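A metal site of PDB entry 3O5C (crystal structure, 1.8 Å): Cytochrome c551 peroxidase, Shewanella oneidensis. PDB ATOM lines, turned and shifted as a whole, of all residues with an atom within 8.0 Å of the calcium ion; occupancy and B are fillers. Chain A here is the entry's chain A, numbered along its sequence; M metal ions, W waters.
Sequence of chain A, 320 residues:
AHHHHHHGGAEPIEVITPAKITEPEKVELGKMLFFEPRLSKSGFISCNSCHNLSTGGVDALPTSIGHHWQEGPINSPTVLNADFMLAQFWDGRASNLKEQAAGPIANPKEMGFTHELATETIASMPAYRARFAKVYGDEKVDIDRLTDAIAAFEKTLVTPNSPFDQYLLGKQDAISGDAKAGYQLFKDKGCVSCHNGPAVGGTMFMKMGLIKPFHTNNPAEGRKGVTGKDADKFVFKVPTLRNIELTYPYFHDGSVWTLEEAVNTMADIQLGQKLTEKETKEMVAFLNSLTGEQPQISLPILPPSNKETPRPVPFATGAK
The side-chain amide nitrogen (ND2) of Asn 75 lies within hydrogen-bond range of the backbone carbonyl oxygen (O) of Leu 61 (2.8 Å). The indole nitrogen of Trp 90 is in hydrogen-bond range of the backbone carbonyl oxygen of Asn 75. The side-chain amide nitrogen of Asn 75 lies within hydrogen-bond range of the backbone carbonyl oxygen of Pro 62. O of His 252 sits at hydrogen-bond distance from N of Asn 75, 2.9 Å away.
Three residues have an atom within 4 Å of the calcium ion: Asn 75, Thr 247 and Pro 249.
The calcium ion is bound by the side-chain amide oxygen of Asn 75 (2.4 Å), the backbone carbonyl oxygen of Pro 249 (2.4 Å), water W2 (2.4 Å), water W1 (2.5 Å), the backbone carbonyl oxygen of Thr 247 (2.5 Å), water W3 (2.5 Å) and water W4 (2.6 Å). The calcium ion has seven donor atoms within binding distance.
Water W2 lies within hydrogen-bond range of the backbone carbonyl oxygen (O) of Tyr 248 and the side-chain amide nitrogen (ND2) of Asn 75.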
ATOM      1  N   VAL A  58       5.860  17.975 -21.832  1.00  0.00           N
ATOM      2  CA  VAL A  58       6.269  17.653 -23.213  1.00  0.00           C
ATOM      3  C   VAL A  58       6.596  18.933 -23.999  1.00  0.00           C
ATOM      4  O   VAL A  58       6.118  20.025 -23.651  1.00  0.00           O
ATOM      5  CB  VAL A  58       5.162  16.895 -23.965  1.00  0.00           C
ATOM      6  CG1 VAL A  58       4.883  15.525 -23.338  1.00  0.00           C
ATOM      7  CG2 VAL A  58       3.845  17.735 -24.048  1.00  0.00           C
ATOM      8  N   ASP A  59       7.373  18.813 -25.085  1.00  0.00           N
ATOM      9  CA  ASP A  59       7.636  19.950 -25.988  1.00  0.00           C
ATOM     10  C   ASP A  59       6.453  20.244 -26.942  1.00  0.00           C
ATOM     11  O   ASP A  59       6.434  21.298 -27.594  1.00  0.00           O
ATOM     12  CB  ASP A  59       8.955  19.808 -26.782  1.00  0.00           C
ATOM     13  CG  ASP A  59       9.124  18.442 -27.448  1.00  0.00           C
ATOM     14  OD1 ASP A  59       8.120  17.831 -27.888  1.00  0.00           O
ATOM     15  OD2 ASP A  59      10.275  17.975 -27.545  1.00  0.00           O
ATOM     16  N   ALA A  60       5.482  19.336 -26.998  1.00  0.00           N
ATOM     17  CA  ALA A  60       4.333  19.471 -27.912  1.00  0.00           C
ATOM     18  C   ALA A  60       4.738  19.674 -29.385  1.00  0.00           C
ATOM     19  O   ALA A  60       4.063  20.376 -30.144  1.00  0.00           O
ATOM     20  CB  ALA A  60       3.410  20.581 -27.452  1.00  0.00           C
ATOM     21  N   LEU A  61       5.866  19.053 -29.758  1.00  0.00           N
ATOM     22  CA  LEU A  61       6.327  19.001 -31.134  1.00  0.00           C
ATOM     23  C   LEU A  61       6.167  17.571 -31.632  1.00  0.00           C
ATOM     24  O   LEU A  61       6.172  16.632 -30.850  1.00  0.00           O
ATOM     25  CB  LEU A  61       7.792  19.456 -31.244  1.00  0.00           C
ATOM     26  CG  LEU A  61       8.054  20.845 -30.627  1.00  0.00           C
ATOM     27  CD1 LEU A  61       9.530  21.229 -30.686  1.00  0.00           C
ATOM     28  CD2 LEU A  61       7.188  21.865 -31.320  1.00  0.00           C
ATOM     29  N   PRO A  62       6.009  17.397 -32.952  1.00  0.00           N
ATOM     30  CA  PRO A  62       5.895  16.034 -33.469  1.00  0.00           C
ATOM     31  C   PRO A  62       7.049  15.130 -33.032  1.00  0.00           C
ATOM     32  O   PRO A  62       6.815  14.005 -32.577  1.00  0.00           O
ATOM     33  CB  PRO A  62       5.868  16.229 -34.991  1.00  0.00           C
ATOM     34  CG  PRO A  62       5.391  17.643 -35.186  1.00  0.00           C
ATOM     35  CD  PRO A  62       5.838  18.432 -33.983  1.00  0.00           C
ATOM     36  N   ASN A  75       8.298  11.075 -30.925  1.00  0.00           N
ATOM     37  CA  ASN A  75       7.556  12.065 -30.116  1.00  0.00           C
ATOM     38  C   ASN A  75       7.960  11.977 -28.651  1.00  0.00           C
ATOM     39  O   ASN A  75       7.987  10.875 -28.077  1.00  0.00           O
ATOM     40  CB  ASN A  75       6.035  11.842 -30.259  1.00  0.00           C
ATOM     41  CG  ASN A  75       5.207  12.957 -29.616  1.00  0.00           C
ATOM     42  OD1 ASN A  75       4.639  12.801 -28.528  1.00  0.00           O
ATOM     43  ND2 ASN A  75       5.141  14.105 -30.285  1.00  0.00           N
ATOM     44  N   SER A  76       8.317  13.119 -28.047  1.00  0.00           N
ATOM     45  CA  SER A  76       8.732  13.109 -26.645  1.00  0.00           C
ATOM     46  C   SER A  76       7.501  12.913 -25.762  1.00  0.00           C
ATOM     47  O   SER A  76       6.551  13.698 -25.854  1.00  0.00           O
ATOM     48  CB  SER A  76       9.461  14.391 -26.244  1.00  0.00           C
ATOM     49  OG  SER A  76       8.586  15.504 -26.278  1.00  0.00           O
ATOM     50  N   PRO A  77       7.518  11.857 -24.922  1.00  0.00           N
ATOM     51  CA  PRO A  77       6.450  11.577 -23.982  1.00  0.00           C
ATOM     52  C   PRO A  77       6.519  12.509 -22.787  1.00  0.00           C
ATOM     53  O   PRO A  77       7.579  13.100 -22.501  1.00  0.00           O
ATOM     54  CB  PRO A  77       6.739  10.140 -23.546  1.00  0.00           C
ATOM     55  CG  PRO A  77       8.207  10.056 -23.584  1.00  0.00           C
ATOM     56  CD  PRO A  77       8.623  10.894 -24.780  1.00  0.00           C
ATOM     57  N   THR A  78       5.408  12.614 -22.097  1.00  0.00           N
ATOM     58  CA  THR A  78       5.341  13.390 -20.868  1.00  0.00           C
ATOM     59  C   THR A  78       6.087  12.726 -19.689  1.00  0.00           C
ATOM     60  O   THR A  78       6.027  11.523 -19.498  1.00  0.00           O
ATOM     61  CB  THR A  78       3.897  13.682 -20.477  1.00  0.00           C
ATOM     62  OG1 THR A  78       3.907  14.539 -19.336  1.00  0.00           O
ATOM     63  CG2 THR A  78       3.103  12.396 -20.168  1.00  0.00           C
ATOM     64  N   TRP A  90       9.467   4.619 -25.367  1.00  0.00           N
ATOM     65  CA  TRP A  90       8.439   3.962 -26.196  1.00  0.00           C
ATOM     66  C   TRP A  90       8.670   2.441 -26.352  1.00  0.00           C
ATOM     67  O   TRP A  90       7.719   1.673 -26.436  1.00  0.00           O
ATOM     68  CB  TRP A  90       8.389   4.617 -27.584  1.00  0.00           C
ATOM     69  CG  TRP A  90       7.623   5.916 -27.640  1.00  0.00           C
ATOM     70  CD1 TRP A  90       8.134   7.179 -27.650  1.00  0.00           C
ATOM     71  CD2 TRP A  90       6.203   6.060 -27.743  1.00  0.00           C
ATOM     72  NE1 TRP A  90       7.136   8.101 -27.744  1.00  0.00           N
ATOM     73  CE2 TRP A  90       5.939   7.435 -27.807  1.00  0.00           C
ATOM     74  CE3 TRP A  90       5.140   5.155 -27.799  1.00  0.00           C
ATOM     75  CZ2 TRP A  90       4.637   7.940 -27.902  1.00  0.00           C
ATOM     76  CZ3 TRP A  90       3.858   5.645 -27.896  1.00  0.00           C
ATOM     77  CH2 TRP A  90       3.609   7.031 -27.945  1.00  0.00           C
ATOM     78  N   PRO A 239       0.850   4.352 -23.876  1.00  0.00           N
ATOM     79  CA  PRO A 239       1.069   5.609 -23.126  1.00  0.00           C
ATOM     80  C   PRO A 239       0.027   5.871 -22.051  1.00  0.00           C
ATOM     81  O   PRO A 239      -1.102   5.336 -22.111  1.00  0.00           O
ATOM     82  CB  PRO A 239       0.998   6.697 -24.207  1.00  0.00           C
ATOM     83  CG  PRO A 239       1.121   5.978 -25.509  1.00  0.00           C
ATOM     84  CD  PRO A 239       0.581   4.608 -25.296  1.00  0.00           C
ATOM     85  N   ILE A 244      -3.768  13.815 -21.412  1.00  0.00           N
ATOM     86  CA  ILE A 244      -3.655  13.619 -22.865  1.00  0.00           C
ATOM     87  C   ILE A 244      -4.121  14.875 -23.604  1.00  0.00           C
ATOM     88  O   ILE A 244      -3.655  15.165 -24.697  1.00  0.00           O
ATOM     89  CB  ILE A 244      -4.388  12.330 -23.316  1.00  0.00           C
ATOM     90  CG1 ILE A 244      -3.992  11.931 -24.752  1.00  0.00           C
ATOM     91  CG2 ILE A 244      -5.888  12.463 -23.183  1.00  0.00           C
ATOM     92  CD1 ILE A 244      -2.547  11.577 -24.885  1.00  0.00           C
ATOM     93  N   LEU A 246      -3.148  17.738 -22.906  1.00  0.00           N
ATOM     94  CA  LEU A 246      -2.009  18.681 -22.916  1.00  0.00           C
ATOM     95  C   LEU A 246      -0.797  18.195 -23.676  1.00  0.00           C
ATOM     96  O   LEU A 246       0.185  18.937 -23.815  1.00  0.00           O
ATOM     97  CB  LEU A 246      -1.549  18.951 -21.489  1.00  0.00           C
ATOM     98  CG  LEU A 246      -2.636  19.314 -20.498  1.00  0.00           C
ATOM     99  CD1 LEU A 246      -1.980  19.477 -19.143  1.00  0.00           C
ATOM    100  CD2 LEU A 246      -3.391  20.606 -20.950  1.00  0.00           C
ATOM    101  N   THR A 247      -0.829  16.953 -24.164  1.00  0.00           N
ATOM    102  CA  THR A 247       0.380  16.352 -24.708  1.00  0.00           C
ATOM    103  C   THR A 247       0.248  16.001 -26.197  1.00  0.00           C
ATOM    104  O   THR A 247       0.877  15.092 -26.661  1.00  0.00           O
ATOM    105  CB  THR A 247       0.799  15.109 -23.891  1.00  0.00           C
ATOM    106  OG1 THR A 247      -0.205  14.098 -24.000  1.00  0.00           O
ATOM    107  CG2 THR A 247       1.004  15.494 -22.410  1.00  0.00           C
ATOM    108  N   TYR A 248      -0.556  16.753 -26.920  1.00  0.00           N
ATOM    109  CA  TYR A 248      -0.527  16.764 -28.386  1.00  0.00           C
ATOM    110  C   TYR A 248       0.891  17.109 -28.893  1.00  0.00           C
ATOM    111  O   TYR A 248       1.697  17.734 -28.175  1.00  0.00           O
ATOM    112  CB  TYR A 248      -1.568  17.774 -28.940  1.00  0.00           C
ATOM    113  CG  TYR A 248      -1.408  19.088 -28.261  1.00  0.00           C
ATOM    114  CD1 TYR A 248      -2.143  19.401 -27.107  1.00  0.00           C
ATOM    115  CD2 TYR A 248      -0.402  19.977 -28.662  1.00  0.00           C
ATOM    116  CE1 TYR A 248      -1.928  20.587 -26.434  1.00  0.00           C
ATOM    117  CE2 TYR A 248      -0.194  21.157 -28.003  1.00  0.00           C
ATOM    118  CZ  TYR A 248      -0.944  21.460 -26.886  1.00  0.00           C
ATOM    119  OH  TYR A 248      -0.710  22.632 -26.214  1.00  0.00           O
ATOM    120  N   PRO A 249       1.227  16.708 -30.127  1.00  0.00           N
ATOM    121  CA  PRO A 249       0.446  15.837 -30.972  1.00  0.00           C
ATOM    122  C   PRO A 249       0.638  14.388 -30.521  1.00  0.00           C
ATOM    123  O   PRO A 249       1.546  14.104 -29.723  1.00  0.00           O
ATOM    124  CB  PRO A 249       1.040  16.075 -32.361  1.00  0.00           C
ATOM    125  CG  PRO A 249       2.471  16.428 -32.074  1.00  0.00           C
ATOM    126  CD  PRO A 249       2.479  17.133 -30.762  1.00  0.00           C
ATOM    127  N   TYR A 250      -0.181  13.501 -31.071  1.00  0.00           N
ATOM    128  CA  TYR A 250      -0.368  12.163 -30.528  1.00  0.00           C
ATOM    129  C   TYR A 250       0.295  11.069 -31.369  1.00  0.00           C
ATOM    130  O   TYR A 250       0.630  11.255 -32.553  1.00  0.00           O
ATOM    131  CB  TYR A 250      -1.872  11.903 -30.342  1.00  0.00           C
ATOM    132  CG  TYR A 250      -2.507  12.957 -29.460  1.00  0.00           C
ATOM    133  CD1 TYR A 250      -2.133  13.080 -28.124  1.00  0.00           C
ATOM    134  CD2 TYR A 250      -3.457  13.847 -29.963  1.00  0.00           C
ATOM    135  CE1 TYR A 250      -2.673  14.049 -27.314  1.00  0.00           C
ATOM    136  CE2 TYR A 250      -4.011  14.824 -29.156  1.00  0.00           C
ATOM    137  CZ  TYR A 250      -3.619  14.912 -27.833  1.00  0.00           C
ATOM    138  OH  TYR A 250      -4.167  15.898 -27.034  1.00  0.00           O
ATOM    139  N   PHE A 251       0.464   9.921 -30.712  1.00  0.00           N
ATOM    140  CA  PHE A 251       1.179   8.762 -31.213  1.00  0.00           C
ATOM    141  C   PHE A 251       2.686   9.018 -31.260  1.00  0.00           C
ATOM    142  O   PHE A 251       3.143  10.146 -31.125  1.00  0.00           O
ATOM    143  CB  PHE A 251       0.618   8.256 -32.543  1.00  0.00           C
ATOM    144  CG  PHE A 251      -0.846   7.962 -32.504  1.00  0.00           C
ATOM    145  CD1 PHE A 251      -1.414   7.323 -31.405  1.00  0.00           C
ATOM    146  CD2 PHE A 251      -1.668   8.338 -33.551  1.00  0.00           C
ATOM    147  CE1 PHE A 251      -2.768   7.054 -31.352  1.00  0.00           C
ATOM    148  CE2 PHE A 251      -3.040   8.063 -33.522  1.00  0.00           C
ATOM    149  CZ  PHE A 251      -3.586   7.426 -32.426  1.00  0.00           C
ATOM    150  N   HIS A 252       3.453   7.947 -31.426  1.00  0.00           N
ATOM    151  CA  HIS A 252       4.909   8.042 -31.344  1.00  0.00           C
ATOM    152  C   HIS A 252       5.484   8.834 -32.520  1.00  0.00           C
ATOM    153  O   HIS A 252       6.597   9.355 -32.453  1.00  0.00           O
ATOM    154  CB  HIS A 252       5.548   6.657 -31.251  1.00  0.00           C
ATOM    155  CG  HIS A 252       5.460   5.860 -32.516  1.00  0.00           C
ATOM    156  ND1 HIS A 252       4.399   5.029 -32.790  1.00  0.00           N
ATOM    157  CD2 HIS A 252       6.306   5.757 -33.572  1.00  0.00           C
ATOM    158  CE1 HIS A 252       4.589   4.443 -33.958  1.00  0.00           C
ATOM    159  NE2 HIS A 252       5.736   4.874 -34.459  1.00  0.00           N
ATOM    160  N   ASP A 253       4.707   8.928 -33.590  1.00  0.00           N
ATOM    161  CA  ASP A 253       5.115   9.732 -34.745  1.00  0.00           C
ATOM    162  C   ASP A 253       4.682  11.196 -34.672  1.00  0.00           C
ATOM    163  O   ASP A 253       5.046  11.976 -35.525  1.00  0.00           O
ATOM    164  CB  ASP A 253       4.696   9.062 -36.074  1.00  0.00           C
ATOM    165  CG  ASP A 253       3.185   9.050 -36.296  1.00  0.00           C
ATOM    166  OD1 ASP A 253       2.401   9.383 -35.379  1.00  0.00           O
ATOM    167  OD2 ASP A 253       2.787   8.725 -37.426  1.00  0.00           O
ATOM    168  N   GLY A 254       3.912  11.569 -33.629  1.00  0.00           N
ATOM    169  CA  GLY A 254       3.434  12.953 -33.462  1.00  0.00           C
ATOM    170  C   GLY A 254       2.663  13.470 -34.663  1.00  0.00           C
ATOM    171  O   GLY A 254       2.843  14.611 -35.108  1.00  0.00           O
ATOM    172  N   SER A 255       1.788  12.623 -35.201  1.00  0.00           N
ATOM    173  CA  SER A 255       1.164  12.872 -36.498  1.00  0.00           C
ATOM    174  C   SER A 255      -0.216  13.496 -36.386  1.00  0.00           C
ATOM    175  O   SER A 255      -0.712  14.080 -37.349  1.00  0.00           O
ATOM    176  CB  SER A 255       1.082  11.575 -37.290  1.00  0.00           C
ATOM    177  OG  SER A 255       0.303  10.596 -36.603  1.00  0.00           O
ATOM    178  N   VAL A 256      -0.832  13.377 -35.218  1.00  0.00           N
ATOM    179  CA  VAL A 256      -2.224  13.754 -35.036  1.00  0.00           C
ATOM    180  C   VAL A 256      -2.349  14.812 -33.924  1.00  0.00           C
ATOM    181  O   VAL A 256      -1.893  14.593 -32.820  1.00  0.00           O
ATOM    182  CB  VAL A 256      -3.039  12.506 -34.701  1.00  0.00           C
ATOM    183  CG1 VAL A 256      -4.433  12.886 -34.375  1.00  0.00           C
ATOM    184  CG2 VAL A 256      -2.997  11.507 -35.866  1.00  0.00           C
HETATM  185 CA    CA M   1       2.548  13.507 -27.640  1.00  0.00          CA
HETATM  186  O   HOH W   1       3.776  13.211 -25.514  1.00  0.00           O
HETATM  187  O   HOH W   2       3.685  15.586 -28.044  1.00  0.00           O
HETATM  188  O   HOH W   3       2.246  11.105 -28.277  1.00  0.00           O
HETATM  189  O   HOH W   4       0.819  12.401 -26.057  1.00  0.00           O
